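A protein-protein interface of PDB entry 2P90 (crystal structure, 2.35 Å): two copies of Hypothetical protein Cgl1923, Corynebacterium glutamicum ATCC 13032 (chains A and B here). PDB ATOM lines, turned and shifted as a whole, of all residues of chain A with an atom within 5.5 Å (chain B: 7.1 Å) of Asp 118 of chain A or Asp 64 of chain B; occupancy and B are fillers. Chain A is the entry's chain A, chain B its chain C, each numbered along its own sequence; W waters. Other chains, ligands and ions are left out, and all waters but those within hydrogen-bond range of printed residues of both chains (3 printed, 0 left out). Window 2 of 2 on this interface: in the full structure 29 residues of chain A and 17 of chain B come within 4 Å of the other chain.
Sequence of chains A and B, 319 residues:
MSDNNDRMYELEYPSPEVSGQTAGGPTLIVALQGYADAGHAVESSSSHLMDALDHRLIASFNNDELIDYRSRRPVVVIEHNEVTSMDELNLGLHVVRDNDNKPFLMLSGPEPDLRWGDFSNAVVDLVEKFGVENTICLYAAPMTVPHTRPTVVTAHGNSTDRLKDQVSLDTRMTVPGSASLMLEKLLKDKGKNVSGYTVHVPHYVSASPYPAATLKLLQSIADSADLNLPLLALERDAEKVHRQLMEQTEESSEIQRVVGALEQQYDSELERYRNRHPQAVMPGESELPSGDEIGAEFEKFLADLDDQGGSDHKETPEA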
ATOM      1  N   ASP A   6     -18.112   3.563   0.830  1.00  0.00           N
ATOM      2  CA  ASP A   6     -17.845   4.596   1.889  1.00  0.00           C
ATOM      3  C   ASP A   6     -18.509   4.218   3.229  1.00  0.00           C
ATOM      4  O   ASP A   6     -17.816   4.068   4.249  1.00  0.00           O
ATOM      5  CB  ASP A   6     -18.301   5.989   1.422  1.00  0.00           C
ATOM      6  CG  ASP A   6     -17.949   7.095   2.424  1.00  0.00           C
ATOM      7  OD1 ASP A   6     -16.762   7.517   2.454  1.00  0.00           O
ATOM      8  OD2 ASP A   6     -18.863   7.547   3.167  1.00  0.00           O
ATOM      9  N   MET A   8     -19.565   1.374   3.461  1.00  0.00           N
ATOM     10  CA  MET A   8     -19.166  -0.013   3.457  1.00  0.00           C
ATOM     11  C   MET A   8     -18.069  -0.329   4.451  1.00  0.00           C
ATOM     12  O   MET A   8     -17.972  -1.452   4.871  1.00  0.00           O
ATOM     13  CB  MET A   8     -18.735  -0.456   2.048  1.00  0.00           C
ATOM     14  CG  MET A   8     -19.852  -0.571   1.000  1.00  0.00           C
ATOM     15  SD  MET A   8     -21.359  -1.462   1.429  1.00  0.00           S
ATOM     16  CE  MET A   8     -22.389  -0.140   2.093  1.00  0.00           C
ATOM     17  N   ARG A 115     -24.973  -6.053  -1.522  1.00  0.00           N
ATOM     18  CA  ARG A 115     -24.388  -4.745  -1.920  1.00  0.00           C
ATOM     19  C   ARG A 115     -23.138  -4.845  -2.758  1.00  0.00           C
ATOM     20  O   ARG A 115     -22.211  -4.064  -2.573  1.00  0.00           O
ATOM     21  CB  ARG A 115     -24.081  -3.854  -0.712  1.00  0.00           C
ATOM     22  CG  ARG A 115     -25.272  -3.480   0.152  1.00  0.00           C
ATOM     23  CD  ARG A 115     -25.241  -1.944   0.392  1.00  0.00           C
ATOM     24  NE  ARG A 115     -26.595  -1.610   0.682  1.00  0.00           N
ATOM     25  CZ  ARG A 115     -27.351  -0.674   0.134  1.00  0.00           C
ATOM     26  NH1 ARG A 115     -26.913   0.229  -0.748  1.00  0.00           N
ATOM     27  NH2 ARG A 115     -28.584  -0.643   0.564  1.00  0.00           N
ATOM     28  N   TRP A 116     -23.122  -5.770  -3.706  1.00  0.00           N
ATOM     29  CA  TRP A 116     -21.956  -5.989  -4.557  1.00  0.00           C
ATOM     30  C   TRP A 116     -21.512  -4.737  -5.292  1.00  0.00           C
ATOM     31  O   TRP A 116     -20.326  -4.542  -5.451  1.00  0.00           O
ATOM     32  CB  TRP A 116     -22.191  -7.150  -5.533  1.00  0.00           C
ATOM     33  CG  TRP A 116     -22.074  -8.516  -4.905  1.00  0.00           C
ATOM     34  CD1 TRP A 116     -22.012  -8.819  -3.539  1.00  0.00           C
ATOM     35  CD2 TRP A 116     -22.097  -9.775  -5.586  1.00  0.00           C
ATOM     36  NE1 TRP A 116     -21.978 -10.179  -3.365  1.00  0.00           N
ATOM     37  CE2 TRP A 116     -22.035 -10.792  -4.588  1.00  0.00           C
ATOM     38  CE3 TRP A 116     -22.184 -10.151  -6.953  1.00  0.00           C
ATOM     39  CZ2 TRP A 116     -22.025 -12.143  -4.909  1.00  0.00           C
ATOM     40  CZ3 TRP A 116     -22.175 -11.478  -7.274  1.00  0.00           C
ATOM     41  CH2 TRP A 116     -22.098 -12.466  -6.258  1.00  0.00           C
ATOM     42  N   GLY A 117     -22.464  -3.912  -5.756  1.00  0.00           N
ATOM     43  CA  GLY A 117     -22.157  -2.666  -6.460  1.00  0.00           C
ATOM     44  C   GLY A 117     -21.406  -1.723  -5.531  1.00  0.00           C
ATOM     45  O   GLY A 117     -20.303  -1.292  -5.867  1.00  0.00           O
ATOM     46  N   ASP A 118     -21.981  -1.423  -4.362  1.00  0.00           N
ATOM     47  CA  ASP A 118     -21.331  -0.587  -3.356  1.00  0.00           C
ATOM     48  C   ASP A 118     -20.004  -1.140  -2.885  1.00  0.00           C
ATOM     49  O   ASP A 118     -19.014  -0.407  -2.796  1.00  0.00           O
ATOM     50  CB  ASP A 118     -22.223  -0.363  -2.152  1.00  0.00           C
ATOM     51  CG  ASP A 118     -23.389   0.540  -2.449  1.00  0.00           C
ATOM     52  OD1 ASP A 118     -23.325   1.356  -3.400  1.00  0.00           O
ATOM     53  OD2 ASP A 118     -24.396   0.426  -1.734  1.00  0.00           O
ATOM     54  N   PHE A 119     -19.985  -2.427  -2.584  1.00  0.00           N
ATOM     55  CA  PHE A 119     -18.770  -3.117  -2.174  1.00  0.00           C
ATOM     56  C   PHE A 119     -17.633  -2.946  -3.188  1.00  0.00           C
ATOM     57  O   PHE A 119     -16.492  -2.626  -2.806  1.00  0.00           O
ATOM     58  CB  PHE A 119     -19.067  -4.607  -1.910  1.00  0.00           C
ATOM     59  CG  PHE A 119     -17.841  -5.420  -1.605  1.00  0.00           C
ATOM     60  CD1 PHE A 119     -17.119  -5.196  -0.442  1.00  0.00           C
ATOM     61  CD2 PHE A 119     -17.379  -6.373  -2.514  1.00  0.00           C
ATOM     62  CE1 PHE A 119     -15.960  -5.907  -0.156  1.00  0.00           C
ATOM     63  CE2 PHE A 119     -16.221  -7.094  -2.253  1.00  0.00           C
ATOM     64  CZ  PHE A 119     -15.503  -6.875  -1.052  1.00  0.00           C
ATOM     65  N   SER A 120     -17.911  -3.159  -4.472  1.00  0.00           N
ATOM     66  CA  SER A 120     -16.828  -3.066  -5.468  1.00  0.00           C
ATOM     67  C   SER A 120     -16.406  -1.623  -5.764  1.00  0.00           C
ATOM     68  O   SER A 120     -15.210  -1.369  -5.935  1.00  0.00           O
ATOM     69  CB  SER A 120     -17.121  -3.887  -6.738  1.00  0.00           C
ATOM     70  OG  SER A 120     -18.360  -3.523  -7.293  1.00  0.00           O
ATOM     71  N   ASN A 121     -17.363  -0.675  -5.806  1.00  0.00           N
ATOM     72  CA  ASN A 121     -17.002   0.748  -5.792  1.00  0.00           C
ATOM     73  C   ASN A 121     -16.065   1.106  -4.602  1.00  0.00           C
ATOM     74  O   ASN A 121     -15.081   1.815  -4.805  1.00  0.00           O
ATOM     75  CB  ASN A 121     -18.211   1.683  -5.744  1.00  0.00           C
ATOM     76  CG  ASN A 121     -19.109   1.610  -6.976  1.00  0.00           C
ATOM     77  OD1 ASN A 121     -18.735   1.115  -8.030  1.00  0.00           O
ATOM     78  ND2 ASN A 121     -20.334   2.128  -6.826  1.00  0.00           N
ATOM     79  N   ALA A 122     -16.381   0.656  -3.380  1.00  0.00           N
ATOM     80  CA  ALA A 122     -15.521   0.875  -2.178  1.00  0.00           C
ATOM     81  C   ALA A 122     -14.131   0.298  -2.342  1.00  0.00           C
ATOM     82  O   ALA A 122     -13.145   0.926  -2.023  1.00  0.00           O
ATOM     83  CB  ALA A 122     -16.164   0.290  -0.895  1.00  0.00           C
ATOM     84  N   VAL A 123     -14.048  -0.904  -2.869  1.00  0.00           N
ATOM     85  CA  VAL A 123     -12.749  -1.499  -3.116  1.00  0.00           C
ATOM     86  C   VAL A 123     -11.935  -0.698  -4.155  1.00  0.00           C
ATOM     87  O   VAL A 123     -10.752  -0.447  -3.927  1.00  0.00           O
ATOM     88  CB  VAL A 123     -12.837  -2.977  -3.470  1.00  0.00           C
ATOM     89  CG1 VAL A 123     -11.413  -3.547  -3.647  1.00  0.00           C
ATOM     90  CG2 VAL A 123     -13.557  -3.720  -2.371  1.00  0.00           C
ATOM     91  N   PHE B  61     -34.814  -0.111 -10.752  1.00  0.00           N
ATOM     92  CA  PHE B  61     -34.684  -0.366  -9.312  1.00  0.00           C
ATOM     93  C   PHE B  61     -33.214  -0.571  -8.889  1.00  0.00           C
ATOM     94  O   PHE B  61     -32.412  -1.016  -9.693  1.00  0.00           O
ATOM     95  CB  PHE B  61     -35.592  -1.530  -8.920  1.00  0.00           C
ATOM     96  CG  PHE B  61     -37.043  -1.139  -8.918  1.00  0.00           C
ATOM     97  CD1 PHE B  61     -37.676  -0.745  -7.713  1.00  0.00           C
ATOM     98  CD2 PHE B  61     -37.757  -1.065 -10.115  1.00  0.00           C
ATOM     99  CE1 PHE B  61     -38.998  -0.357  -7.707  1.00  0.00           C
ATOM    100  CE2 PHE B  61     -39.104  -0.658 -10.114  1.00  0.00           C
ATOM    101  CZ  PHE B  61     -39.720  -0.301  -8.895  1.00  0.00           C
ATOM    102  N   ASN B  62     -32.881  -0.237  -7.643  1.00  0.00           N
ATOM    103  CA  ASN B  62     -31.508  -0.392  -7.136  1.00  0.00           C
ATOM    104  C   ASN B  62     -31.249  -1.818  -6.627  1.00  0.00           C
ATOM    105  O   ASN B  62     -31.737  -2.222  -5.568  1.00  0.00           O
ATOM    106  CB  ASN B  62     -31.232   0.630  -6.014  1.00  0.00           C
ATOM    107  CG  ASN B  62     -29.722   0.704  -5.618  1.00  0.00           C
ATOM    108  OD1 ASN B  62     -28.912  -0.188  -5.946  1.00  0.00           O
ATOM    109  ND2 ASN B  62     -29.350   1.776  -4.903  1.00  0.00           N
ATOM    110  N   ASN B  63     -30.488  -2.593  -7.371  1.00  0.00           N
ATOM    111  CA  ASN B  63     -30.222  -3.965  -6.928  1.00  0.00           C
ATOM    112  C   ASN B  63     -29.448  -4.048  -5.620  1.00  0.00           C
ATOM    113  O   ASN B  63     -29.545  -5.044  -4.914  1.00  0.00           O
ATOM    114  CB  ASN B  63     -29.492  -4.762  -8.012  1.00  0.00           C
ATOM    115  CG  ASN B  63     -30.422  -5.246  -9.106  1.00  0.00           C
ATOM    116  OD1 ASN B  63     -31.646  -5.005  -9.078  1.00  0.00           O
ATOM    117  ND2 ASN B  63     -29.853  -5.966 -10.069  1.00  0.00           N
ATOM    118  N   ASP B  64     -28.705  -3.006  -5.262  1.00  0.00           N
ATOM    119  CA  ASP B  64     -28.065  -3.021  -3.938  1.00  0.00           C
ATOM    120  C   ASP B  64     -29.045  -2.986  -2.765  1.00  0.00           C
ATOM    121  O   ASP B  64     -28.747  -3.598  -1.752  1.00  0.00           O
ATOM    122  CB  ASP B  64     -26.939  -1.994  -3.793  1.00  0.00           C
ATOM    123  CG  ASP B  64     -25.632  -2.446  -4.477  1.00  0.00           C
ATOM    124  OD1 ASP B  64     -25.518  -3.546  -5.113  1.00  0.00           O
ATOM    125  OD2 ASP B  64     -24.682  -1.678  -4.365  1.00  0.00           O
ATOM    126  N   GLU B  65     -30.225  -2.360  -2.933  1.00  0.00           N
ATOM    127  CA  GLU B  65     -31.324  -2.370  -1.908  1.00  0.00           C
ATOM    128  C   GLU B  65     -32.134  -3.691  -1.884  1.00  0.00           C
ATOM    129  O   GLU B  65     -32.765  -4.048  -0.893  1.00  0.00           O
ATOM    130  CB  GLU B  65     -32.294  -1.186  -2.127  1.00  0.00           C
ATOM    131  CG  GLU B  65     -31.622   0.196  -2.071  1.00  0.00           C
ATOM    132  CD  GLU B  65     -31.119   0.501  -0.681  1.00  0.00           C
ATOM    133  OE1 GLU B  65     -31.825   0.168   0.290  1.00  0.00           O
ATOM    134  OE2 GLU B  65     -30.014   1.075  -0.543  1.00  0.00           O
ATOM    135  N   LEU B  66     -32.087  -4.430  -2.987  1.00  0.00           N
ATOM    136  CA  LEU B  66     -33.097  -5.429  -3.253  1.00  0.00           C
ATOM    137  C   LEU B  66     -32.605  -6.862  -3.425  1.00  0.00           C
ATOM    138  O   LEU B  66     -33.404  -7.775  -3.367  1.00  0.00           O
ATOM    139  CB  LEU B  66     -33.922  -4.983  -4.490  1.00  0.00           C
ATOM    140  CG  LEU B  66     -34.749  -3.687  -4.275  1.00  0.00           C
ATOM    141  CD1 LEU B  66     -35.260  -3.147  -5.587  1.00  0.00           C
ATOM    142  CD2 LEU B  66     -35.915  -3.860  -3.265  1.00  0.00           C
ATOM    143  N   ILE B  67     -31.308  -7.053  -3.659  1.00  0.00           N
ATOM    144  CA  ILE B  67     -30.791  -8.354  -4.104  1.00  0.00           C
ATOM    145  C   ILE B  67     -29.795  -8.949  -3.090  1.00  0.00           C
ATOM    146  O   ILE B  67     -28.915  -8.246  -2.602  1.00  0.00           O
ATOM    147  CB  ILE B  67     -30.129  -8.316  -5.546  1.00  0.00           C
ATOM    148  CG1 ILE B  67     -31.124  -7.941  -6.653  1.00  0.00           C
ATOM    149  CG2 ILE B  67     -29.478  -9.688  -5.919  1.00  0.00           C
ATOM    150  CD1 ILE B  67     -32.353  -8.869  -6.789  1.00  0.00           C
ATOM    151  N   ASP B  68     -30.000 -10.235  -2.762  1.00  0.00           N
ATOM    152  CA  ASP B  68     -29.000 -11.081  -2.147  1.00  0.00           C
ATOM    153  C   ASP B  68     -28.197 -11.769  -3.287  1.00  0.00           C
ATOM    154  O   ASP B  68     -28.631 -12.782  -3.866  1.00  0.00           O
ATOM    155  CB  ASP B  68     -29.654 -12.120  -1.224  1.00  0.00           C
ATOM    156  CG  ASP B  68     -28.628 -13.063  -0.559  1.00  0.00           C
ATOM    157  OD1 ASP B  68     -27.563 -13.352  -1.154  1.00  0.00           O
ATOM    158  OD2 ASP B  68     -28.878 -13.549   0.576  1.00  0.00           O
ATOM    159  N   TYR B  69     -27.027 -11.211  -3.579  1.00  0.00           N
ATOM    160  CA  TYR B  69     -26.291 -11.595  -4.743  1.00  0.00           C
ATOM    161  C   TYR B  69     -25.688 -12.982  -4.617  1.00  0.00           C
ATOM    162  O   TYR B  69     -25.589 -13.663  -5.620  1.00  0.00           O
ATOM    163  CB  TYR B  69     -25.186 -10.600  -5.006  1.00  0.00           C
ATOM    164  CG  TYR B  69     -25.576  -9.224  -5.443  1.00  0.00           C
ATOM    165  CD1 TYR B  69     -25.611  -8.901  -6.791  1.00  0.00           C
ATOM    166  CD2 TYR B  69     -25.858  -8.220  -4.502  1.00  0.00           C
ATOM    167  CE1 TYR B  69     -25.951  -7.606  -7.225  1.00  0.00           C
ATOM    168  CE2 TYR B  69     -26.208  -6.918  -4.916  1.00  0.00           C
ATOM    169  CZ  TYR B  69     -26.244  -6.623  -6.264  1.00  0.00           C
ATOM    170  OH  TYR B  69     -26.549  -5.356  -6.687  1.00  0.00           O
ATOM    171  N   LEU B 114     -35.093  -8.685  -1.039  1.00  0.00           N
ATOM    172  CA  LEU B 114     -35.123  -7.820   0.144  1.00  0.00           C
ATOM    173  C   LEU B 114     -36.183  -6.794   0.053  1.00  0.00           C
ATOM    174  O   LEU B 114     -36.723  -6.548  -1.029  1.00  0.00           O
ATOM    175  CB  LEU B 114     -33.759  -7.115   0.296  1.00  0.00           C
ATOM    176  CG  LEU B 114     -32.541  -8.061   0.313  1.00  0.00           C
ATOM    177  CD1 LEU B 114     -31.193  -7.370   0.456  1.00  0.00           C
ATOM    178  CD2 LEU B 114     -32.739  -9.155   1.392  1.00  0.00           C
HETATM  179  O   HOH W   1     -29.229   1.703   2.270  1.00  0.00           O
HETATM  180  O   HOH W   2     -30.855  -1.546   2.238  1.00  0.00           O
HETATM  181  O   HOH W   3     -28.012  -6.057  -1.557  1.00  0.00           O
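No position is printed for both chains.
Asp 118 of chain A touches just one residue of chain B: Asp 64 (2.7 Å).
Asp 64 of chain B touches just these residues of chain A: Arg 115, Trp 116, Gly 117 and Asp 118.
Of the printed residues of chain B, Gly 117 of chain A touches Asp 64.
Of the printed residues of chain B, Trp 116 of chain A touches Asp 64 (3.6 Å) and Tyr 69 (3.2 Å).
Printed residues of chain A within 4 Å of Tyr 69 of chain B: Arg 115 and Trp 116.
Of the printed residues of chain A, Glu 65 of chain B touches Arg 115.
Ala 122 of chain A touches none of the printed residues of chain B.
Leu 114 of chain B touches none of the printed residues of chain A.
The nearest printed residue of chain A that does not touch Glu 65 of chain B is Asp 118 of chain A (5.8 Å).
Water W3 lies within hydrogen-bond range of the backbone carbonyl oxygen (O) of Asp 64 of chain B (2.6 Å), the backbone carbonyl oxygen (O) of Ile 67 of chain B (2.6 Å) and the backbone NH (N) of Arg 115 of chain A (3.0 Å).
Water W2 lies within hydrogen-bond range of the side-chain carboxylate (OE1) of Glu 65 of chain B (2.8 Å) and the guanidinium group (NH2) of Arg 115 of chain A (3.0 Å).
Water W1 bridges NH2 of Arg 115 of chain A (3.0 Å) and OE2 of Glu 65 of chain B (3.0 Å).
Among the printed residues, pairs that only touch across the chains: Arg 115 of chain A with Asp 64 of chain B, Arg 115 of chain A with Tyr 69 of chain B, Trp 116 of chain A with Asp 64 of chain B and Trp 116 of chain A with Tyr 69 of chain B.
Of the 11 printed residues of chain A, 4 touch a printed residue of chain B.
Hydrophobic or aromatic side chains of chain A within 4 Å of the printed part of chain B: Trp 116.
Among the printed residues, 7 pairs touch across the chains.
Among the printed residues, Asp or Glu carboxylates within 4 Å of a Lys or Arg side-chain nitrogen of the other chain: Arg 115 of chain A with Glu 65 of chain B.
The guanidinium group (NH2) of Arg 115 of chain A lies within salt-bridge range of the side-chain carboxylate (OE2) of Glu 65 of chain B, at 2.5 Å.
The backbone NH (N) of Gly 117 of chain A sits at hydrogen-bond distance from the side-chain carboxylate (OD1) of Asp 64 of chain B, at 3.1 Å.
The backbone NH of Asp 118 of chain A lies within hydrogen-bond range of the side-chain carboxylate of Asp 64 of chain B, at 2.7 Å.
OD2 of Asp 118 of chain A lies within salt-bridge range of NH1 of Arg 115 of chain A.
O of Trp 116 of chain A lies within hydrogen-bond range of OG of Ser 120 of chain A (2.9 Å).
OG of Ser 120 of chain A is in hydrogen-bond range of O of Gly 117 of chain A.
The side-chain amide oxygen (OD1) of Asn 62 of chain B sits at hydrogen-bond distance from the backbone NH (N) of Asp 64 of chain B.
The side-chain hydroxyl (OH) of Tyr 69 of chain B sits close to the backbone carbonyl oxygen (O) of Asn 63 of chain B (3.5 Å).
OD1 of Asp 64 of chain B lies within hydrogen-bond range of OH of Tyr 69 of chain B, at 2.6 Å.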
